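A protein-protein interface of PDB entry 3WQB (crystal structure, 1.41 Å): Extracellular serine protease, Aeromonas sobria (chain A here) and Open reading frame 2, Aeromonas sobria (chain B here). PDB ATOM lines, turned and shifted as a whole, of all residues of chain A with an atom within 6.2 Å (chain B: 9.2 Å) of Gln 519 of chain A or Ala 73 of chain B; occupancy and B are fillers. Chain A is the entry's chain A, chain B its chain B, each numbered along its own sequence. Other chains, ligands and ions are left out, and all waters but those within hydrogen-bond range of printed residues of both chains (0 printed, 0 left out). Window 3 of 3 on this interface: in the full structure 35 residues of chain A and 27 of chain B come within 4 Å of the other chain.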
ATOM      1  N   ALA A 225      21.495   6.125  21.205  1.00  0.00           N
ATOM      2  CA  ALA A 225      21.782   4.776  20.764  1.00  0.00           C
ATOM      3  C   ALA A 225      20.631   4.278  19.906  1.00  0.00           C
ATOM      4  O   ALA A 225      19.471   4.277  20.345  1.00  0.00           O
ATOM      5  CB  ALA A 225      21.986   3.863  21.971  1.00  0.00           C
ATOM      6  N   GLY A 226      20.961   3.874  18.680  1.00  0.00           N
ATOM      7  CA  GLY A 226      20.003   3.282  17.746  1.00  0.00           C
ATOM      8  C   GLY A 226      18.712   4.064  17.578  1.00  0.00           C
ATOM      9  O   GLY A 226      17.624   3.493  17.652  1.00  0.00           O
ATOM     10  N   TYR A 228      17.350   6.301  19.535  1.00  0.00           N
ATOM     11  CA  TYR A 228      16.728   6.719  20.800  1.00  0.00           C
ATOM     12  C   TYR A 228      17.691   7.574  21.605  1.00  0.00           C
ATOM     13  O   TYR A 228      18.905   7.395  21.526  1.00  0.00           O
ATOM     14  CB  TYR A 228      16.322   5.511  21.653  1.00  0.00           C
ATOM     15  CG  TYR A 228      15.136   4.733  21.124  1.00  0.00           C
ATOM     16  CD1 TYR A 228      15.289   3.813  20.085  1.00  0.00           C
ATOM     17  CD2 TYR A 228      13.860   4.910  21.670  1.00  0.00           C
ATOM     18  CE1 TYR A 228      14.203   3.093  19.593  1.00  0.00           C
ATOM     19  CE2 TYR A 228      12.764   4.189  21.188  1.00  0.00           C
ATOM     20  CZ  TYR A 228      12.944   3.285  20.150  1.00  0.00           C
ATOM     21  OH  TYR A 228      11.870   2.572  19.668  1.00  0.00           O
ATOM     22  N   SER A 514      16.159  -3.297  32.409  1.00  0.00           N
ATOM     23  CA  SER A 514      14.832  -2.699  32.486  1.00  0.00           C
ATOM     24  C   SER A 514      14.228  -2.504  31.098  1.00  0.00           C
ATOM     25  O   SER A 514      13.038  -2.765  30.890  1.00  0.00           O
ATOM     26  CB  SER A 514      14.873  -1.377  33.253  1.00  0.00           C
ATOM     27  OG  SER A 514      15.217  -1.607  34.607  1.00  0.00           O
ATOM     28  N   LEU A 515      15.052  -2.069  30.143  1.00  0.00           N
ATOM     29  CA  LEU A 515      14.581  -1.863  28.779  1.00  0.00           C
ATOM     30  C   LEU A 515      14.123  -3.182  28.164  1.00  0.00           C
ATOM     31  O   LEU A 515      13.065  -3.241  27.532  1.00  0.00           O
ATOM     32  CB  LEU A 515      15.658  -1.194  27.920  1.00  0.00           C
ATOM     33  CG  LEU A 515      15.233  -0.720  26.527  1.00  0.00           C
ATOM     34  CD1 LEU A 515      14.115   0.331  26.591  1.00  0.00           C
ATOM     35  CD2 LEU A 515      16.437  -0.184  25.788  1.00  0.00           C
ATOM     36  N   ASP A 516      14.910  -4.237  28.369  1.00  0.00           N
ATOM     37  CA  ASP A 516      14.563  -5.577  27.894  1.00  0.00           C
ATOM     38  C   ASP A 516      13.241  -6.059  28.474  1.00  0.00           C
ATOM     39  O   ASP A 516      12.404  -6.585  27.744  1.00  0.00           O
ATOM     40  CB  ASP A 516      15.671  -6.580  28.215  1.00  0.00           C
ATOM     41  CG  ASP A 516      16.754  -6.629  27.151  1.00  0.00           C
ATOM     42  OD1 ASP A 516      16.769  -5.763  26.248  1.00  0.00           O
ATOM     43  OD2 ASP A 516      17.598  -7.547  27.223  1.00  0.00           O
ATOM     44  N   GLN A 517      13.051  -5.863  29.778  1.00  0.00           N
ATOM     45  CA  GLN A 517      11.807  -6.267  30.438  1.00  0.00           C
ATOM     46  C   GLN A 517      10.587  -5.541  29.857  1.00  0.00           C
ATOM     47  O   GLN A 517       9.562  -6.170  29.573  1.00  0.00           O
ATOM     48  CB  GLN A 517      11.905  -6.065  31.955  1.00  0.00           C
ATOM     49  CG  GLN A 517      10.711  -6.607  32.751  1.00  0.00           C
ATOM     50  CD  GLN A 517      10.432  -8.080  32.493  1.00  0.00           C
ATOM     51  OE1 GLN A 517       9.318  -8.450  32.121  1.00  0.00           O
ATOM     52  NE2 GLN A 517      11.441  -8.924  32.688  1.00  0.00           N
ATOM     53  N   GLN A 518      10.708  -4.228  29.668  1.00  0.00           N
ATOM     54  CA  GLN A 518       9.639  -3.415  29.080  1.00  0.00           C
ATOM     55  C   GLN A 518       9.346  -3.783  27.623  1.00  0.00           C
ATOM     56  O   GLN A 518       8.188  -4.000  27.252  1.00  0.00           O
ATOM     57  CB  GLN A 518       9.970  -1.921  29.192  1.00  0.00           C
ATOM     58  CG  GLN A 518       8.994  -1.001  28.460  1.00  0.00           C
ATOM     59  CD  GLN A 518       9.389   0.459  28.545  1.00  0.00           C
ATOM     60  OE1 GLN A 518       9.089   1.141  29.528  1.00  0.00           O
ATOM     61  NE2 GLN A 518      10.059   0.953  27.508  1.00  0.00           N
ATOM     62  N   GLN A 519      10.395  -3.858  26.808  1.00  0.00           N
ATOM     63  CA  GLN A 519      10.246  -4.042  25.360  1.00  0.00           C
ATOM     64  C   GLN A 519       9.982  -5.490  24.945  1.00  0.00           C
ATOM     65  O   GLN A 519       9.252  -5.739  23.980  1.00  0.00           O
ATOM     66  CB  GLN A 519      11.487  -3.522  24.620  1.00  0.00           C
ATOM     67  CG  GLN A 519      11.778  -2.037  24.805  1.00  0.00           C
ATOM     68  CD  GLN A 519      10.948  -1.145  23.903  1.00  0.00           C
ATOM     69  OE1 GLN A 519      10.859  -1.371  22.694  1.00  0.00           O
ATOM     70  NE2 GLN A 519      10.348  -0.113  24.486  1.00  0.00           N
ATOM     71  N   LEU A 520      10.577  -6.436  25.670  1.00  0.00           N
ATOM     72  CA  LEU A 520      10.627  -7.839  25.241  1.00  0.00           C
ATOM     73  C   LEU A 520       9.888  -8.801  26.171  1.00  0.00           C
ATOM     74  O   LEU A 520       9.404  -9.844  25.725  1.00  0.00           O
ATOM     75  CB  LEU A 520      12.086  -8.293  25.104  1.00  0.00           C
ATOM     76  CG  LEU A 520      12.933  -8.067  23.843  1.00  0.00           C
ATOM     77  CD1 LEU A 520      12.765  -6.688  23.209  1.00  0.00           C
ATOM     78  CD2 LEU A 520      14.399  -8.321  24.178  1.00  0.00           C
ATOM     79  N   GLY A 521       9.817  -8.458  27.455  1.00  0.00           N
ATOM     80  CA  GLY A 521       9.201  -9.322  28.467  1.00  0.00           C
ATOM     81  C   GLY A 521      10.150 -10.331  29.096  1.00  0.00           C
ATOM     82  O   GLY A 521       9.731 -11.184  29.881  1.00  0.00           O
ATOM     83  N   ARG A 524      17.895 -10.302  28.874  1.00  0.00           N
ATOM     84  CA  ARG A 524      19.057 -10.972  28.293  1.00  0.00           C
ATOM     85  C   ARG A 524      20.297 -10.872  29.192  1.00  0.00           C
ATOM     86  O   ARG A 524      21.107 -11.802  29.251  1.00  0.00           O
ATOM     87  CB  ARG A 524      19.354 -10.404  26.900  1.00  0.00           C
ATOM     88  CG  ARG A 524      18.234 -10.633  25.888  1.00  0.00           C
ATOM     89  CD  ARG A 524      18.563 -10.057  24.521  1.00  0.00           C
ATOM     90  NE  ARG A 524      18.191  -8.649  24.398  1.00  0.00           N
ATOM     91  CZ  ARG A 524      19.053  -7.643  24.284  1.00  0.00           C
ATOM     92  NH1 ARG A 524      20.361  -7.870  24.266  1.00  0.00           N
ATOM     93  NH2 ARG A 524      18.603  -6.399  24.180  1.00  0.00           N
ATOM     94  N   LEU A 563      12.886   7.979  27.649  1.00  0.00           N
ATOM     95  CA  LEU A 563      13.250   7.410  26.361  1.00  0.00           C
ATOM     96  C   LEU A 563      12.616   8.235  25.249  1.00  0.00           C
ATOM     97  O   LEU A 563      11.389   8.372  25.194  1.00  0.00           O
ATOM     98  CB  LEU A 563      12.767   5.959  26.249  1.00  0.00           C
ATOM     99  CG  LEU A 563      13.018   4.973  27.388  1.00  0.00           C
ATOM    100  CD1 LEU A 563      12.141   3.752  27.210  1.00  0.00           C
ATOM    101  CD2 LEU A 563      14.480   4.586  27.399  1.00  0.00           C
ATOM    102  N   THR A 572       8.788   7.831  26.086  1.00  0.00           N
ATOM    103  CA  THR A 572       8.378   6.740  26.966  1.00  0.00           C
ATOM    104  C   THR A 572       9.098   6.927  28.301  1.00  0.00           C
ATOM    105  O   THR A 572      10.160   7.553  28.364  1.00  0.00           O
ATOM    106  CB  THR A 572       8.792   5.350  26.381  1.00  0.00           C
ATOM    107  OG1 THR A 572       8.440   5.267  24.996  1.00  0.00           O
ATOM    108  CG2 THR A 572       8.112   4.202  27.130  1.00  0.00           C
ATOM    109  N   LEU B  40      17.501 -10.434  17.544  1.00  0.00           N
ATOM    110  CA  LEU B  40      16.143 -10.564  17.032  1.00  0.00           C
ATOM    111  C   LEU B  40      16.142 -10.463  15.508  1.00  0.00           C
ATOM    112  O   LEU B  40      16.739  -9.544  14.939  1.00  0.00           O
ATOM    113  CB  LEU B  40      15.229  -9.496  17.649  1.00  0.00           C
ATOM    114  CG  LEU B  40      15.151  -9.393  19.177  1.00  0.00           C
ATOM    115  CD1 LEU B  40      14.493  -8.081  19.591  1.00  0.00           C
ATOM    116  CD2 LEU B  40      14.420 -10.584  19.792  1.00  0.00           C
ATOM    117  N   MET B  70      18.345  -7.174  15.047  1.00  0.00           N
ATOM    118  CA  MET B  70      18.070  -6.132  16.030  1.00  0.00           C
ATOM    119  C   MET B  70      18.487  -6.648  17.406  1.00  0.00           C
ATOM    120  O   MET B  70      18.169  -7.784  17.764  1.00  0.00           O
ATOM    121  CB  MET B  70      16.586  -5.765  16.010  1.00  0.00           C
ATOM    122  CG  MET B  70      16.305  -4.278  16.220  1.00  0.00           C
ATOM    123  SD  MET B  70      14.566  -3.894  16.527  1.00  0.00           S
ATOM    124  CE  MET B  70      13.800  -4.400  14.981  1.00  0.00           C
ATOM    125  N   GLN B  71      19.211  -5.827  18.166  1.00  0.00           N
ATOM    126  CA  GLN B  71      19.729  -6.239  19.480  1.00  0.00           C
ATOM    127  C   GLN B  71      18.969  -5.556  20.614  1.00  0.00           C
ATOM    128  O   GLN B  71      19.571  -4.897  21.470  1.00  0.00           O
ATOM    129  CB  GLN B  71      21.220  -5.910  19.624  1.00  0.00           C
ATOM    130  CG  GLN B  71      21.883  -5.289  18.406  1.00  0.00           C
ATOM    131  CD  GLN B  71      23.171  -4.560  18.755  1.00  0.00           C
ATOM    132  OE1 GLN B  71      23.490  -3.525  18.169  1.00  0.00           O
ATOM    133  NE2 GLN B  71      23.920  -5.101  19.712  1.00  0.00           N
ATOM    134  N   GLY B  72      17.651  -5.723  20.629  1.00  0.00           N
ATOM    135  CA  GLY B  72      16.804  -4.944  21.526  1.00  0.00           C
ATOM    136  C   GLY B  72      16.516  -3.598  20.893  1.00  0.00           C
ATOM    137  O   GLY B  72      16.836  -3.380  19.718  1.00  0.00           O
ATOM    138  N   ALA B  73      15.934  -2.688  21.672  1.00  0.00           N
ATOM    139  CA  ALA B  73      15.422  -1.432  21.125  1.00  0.00           C
ATOM    140  C   ALA B  73      16.146  -0.150  21.567  1.00  0.00           C
ATOM    141  O   ALA B  73      15.565   0.936  21.524  1.00  0.00           O
ATOM    142  CB  ALA B  73      13.913  -1.322  21.386  1.00  0.00           C
ATOM    143  N   ALA B  74      17.403  -0.274  21.992  1.00  0.00           N
ATOM    144  CA  ALA B  74      18.263   0.896  22.203  1.00  0.00           C
ATOM    145  C   ALA B  74      19.649   0.666  21.601  1.00  0.00           C
ATOM    146  O   ALA B  74      20.669   1.077  22.159  1.00  0.00           O
ATOM    147  CB  ALA B  74      18.364   1.241  23.675  1.00  0.00           C
ATOM    148  N   SER B  75      19.665   0.011  20.448  1.00  0.00           N
ATOM    149  CA  SER B  75      20.902  -0.343  19.767  1.00  0.00           C
ATOM    150  C   SER B  75      20.729  -0.239  18.252  1.00  0.00           C
ATOM    151  O   SER B  75      19.606  -0.341  17.747  1.00  0.00           O
ATOM    152  CB  SER B  75      21.340  -1.751  20.171  1.00  0.00           C
ATOM    153  OG  SER B  75      20.252  -2.655  20.115  1.00  0.00           O
ATOM    154  N   PRO B  76      21.840  -0.021  17.522  1.00  0.00           N
ATOM    155  CA  PRO B  76      21.751   0.100  16.071  1.00  0.00           C
ATOM    156  C   PRO B  76      21.407  -1.222  15.402  1.00  0.00           C
ATOM    157  O   PRO B  76      21.721  -2.294  15.927  1.00  0.00           O
ATOM    158  CB  PRO B  76      23.164   0.545  15.667  1.00  0.00           C
ATOM    159  CG  PRO B  76      24.038   0.054  16.762  1.00  0.00           C
ATOM    160  CD  PRO B  76      23.220   0.185  18.003  1.00  0.00           C
ATOM    161  N   GLU B  77      20.746  -1.116  14.256  1.00  0.00           N
ATOM    162  CA  GLU B  77      20.486  -2.237  13.370  1.00  0.00           C
ATOM    163  C   GLU B  77      21.815  -2.831  12.895  1.00  0.00           C
ATOM    164  O   GLU B  77      22.678  -2.105  12.395  1.00  0.00           O
ATOM    165  CB  GLU B  77      19.671  -1.729  12.179  1.00  0.00           C
ATOM    166  CG  GLU B  77      19.181  -2.774  11.224  1.00  0.00           C
ATOM    167  CD  GLU B  77      18.424  -2.161  10.065  1.00  0.00           C
ATOM    168  OE1 GLU B  77      19.073  -1.741   9.081  1.00  0.00           O
ATOM    169  OE2 GLU B  77      17.179  -2.096  10.142  1.00  0.00           O
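Ala 74 of chain B touches Ala 225 of chain A (O to CB, 3.1 Å).
Gly 226 of chain A touches Ser 75 of chain B (CA to C, 3.6 Å).
Gly 226 of chain A touches Pro 76 of chain B (CA to N, 3.8 Å).
Tyr 228 of chain A touches Ala 73 of chain B.
Leu 515 of chain A touches Ala 74 of chain B (CD2 to CB, 3.2 Å).
Ala 73 of chain B touches Gln 519 of chain A.
Arg 524 of chain A touches Gly 72 of chain B (NH2 to CA, 3.5 Å).
The guanidinium group (NH2) of Arg 524 of chain A sits at hydrogen-bond distance from the backbone carbonyl oxygen (O) of Gln 71 of chain B (3.2 Å).
O of Gln 71 of chain B sits at hydrogen-bond distance from OG of Ser 75 of chain B (2.7 Å).
NE2 of Gln 518 of chain A lies close to NE2 of Gln 519 of chain A.
The backbone carbonyl oxygen (O) of Pro 76 of chain B sits close to the side-chain amide oxygen (OE1) of Gln 71 of chain B, 3.1 Å away.
The guanidinium group (NH2) of Arg 524 of chain A lies within salt-bridge range of the side-chain carboxylate (OD1) of Asp 516 of chain A (2.8 Å).
Asp 516 of chain A touches none of the printed residues of chain B.
Gln 519 of chain A touches just one residue of chain B: Ala 73.
Of the printed residues of chain A, Gln 71 of chain B touches Arg 524.
Of the printed residues of chain A, Ala 73 of chain B touches Tyr 228 (3.2 Å) and Gln 519 (3.3 Å).
Of the printed residues of chain A, Ser 75 of chain B touches Gly 226.
The nearest residue of chain B that does not touch Gln 519 of chain A is Gly 72 of chain B (6.3 Å).
The nearest residue of chain A that does not touch Ala 73 of chain B is Leu 515 of chain A (4.2 Å).
Of the 14 printed residues of chain A, 6 touch a printed residue of chain B.
Printed residues of chain B that touch a printed residue of chain A: Gln 71, Gly 72, Ala 73, Ala 74, Ser 75 and Pro 76.
Among the printed residues, 8 pairs touch across the chains.
Among the printed residues, no Asp or Glu carboxylate lies within 4 Å of a Lys or Arg side-chain nitrogen of the other chain.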
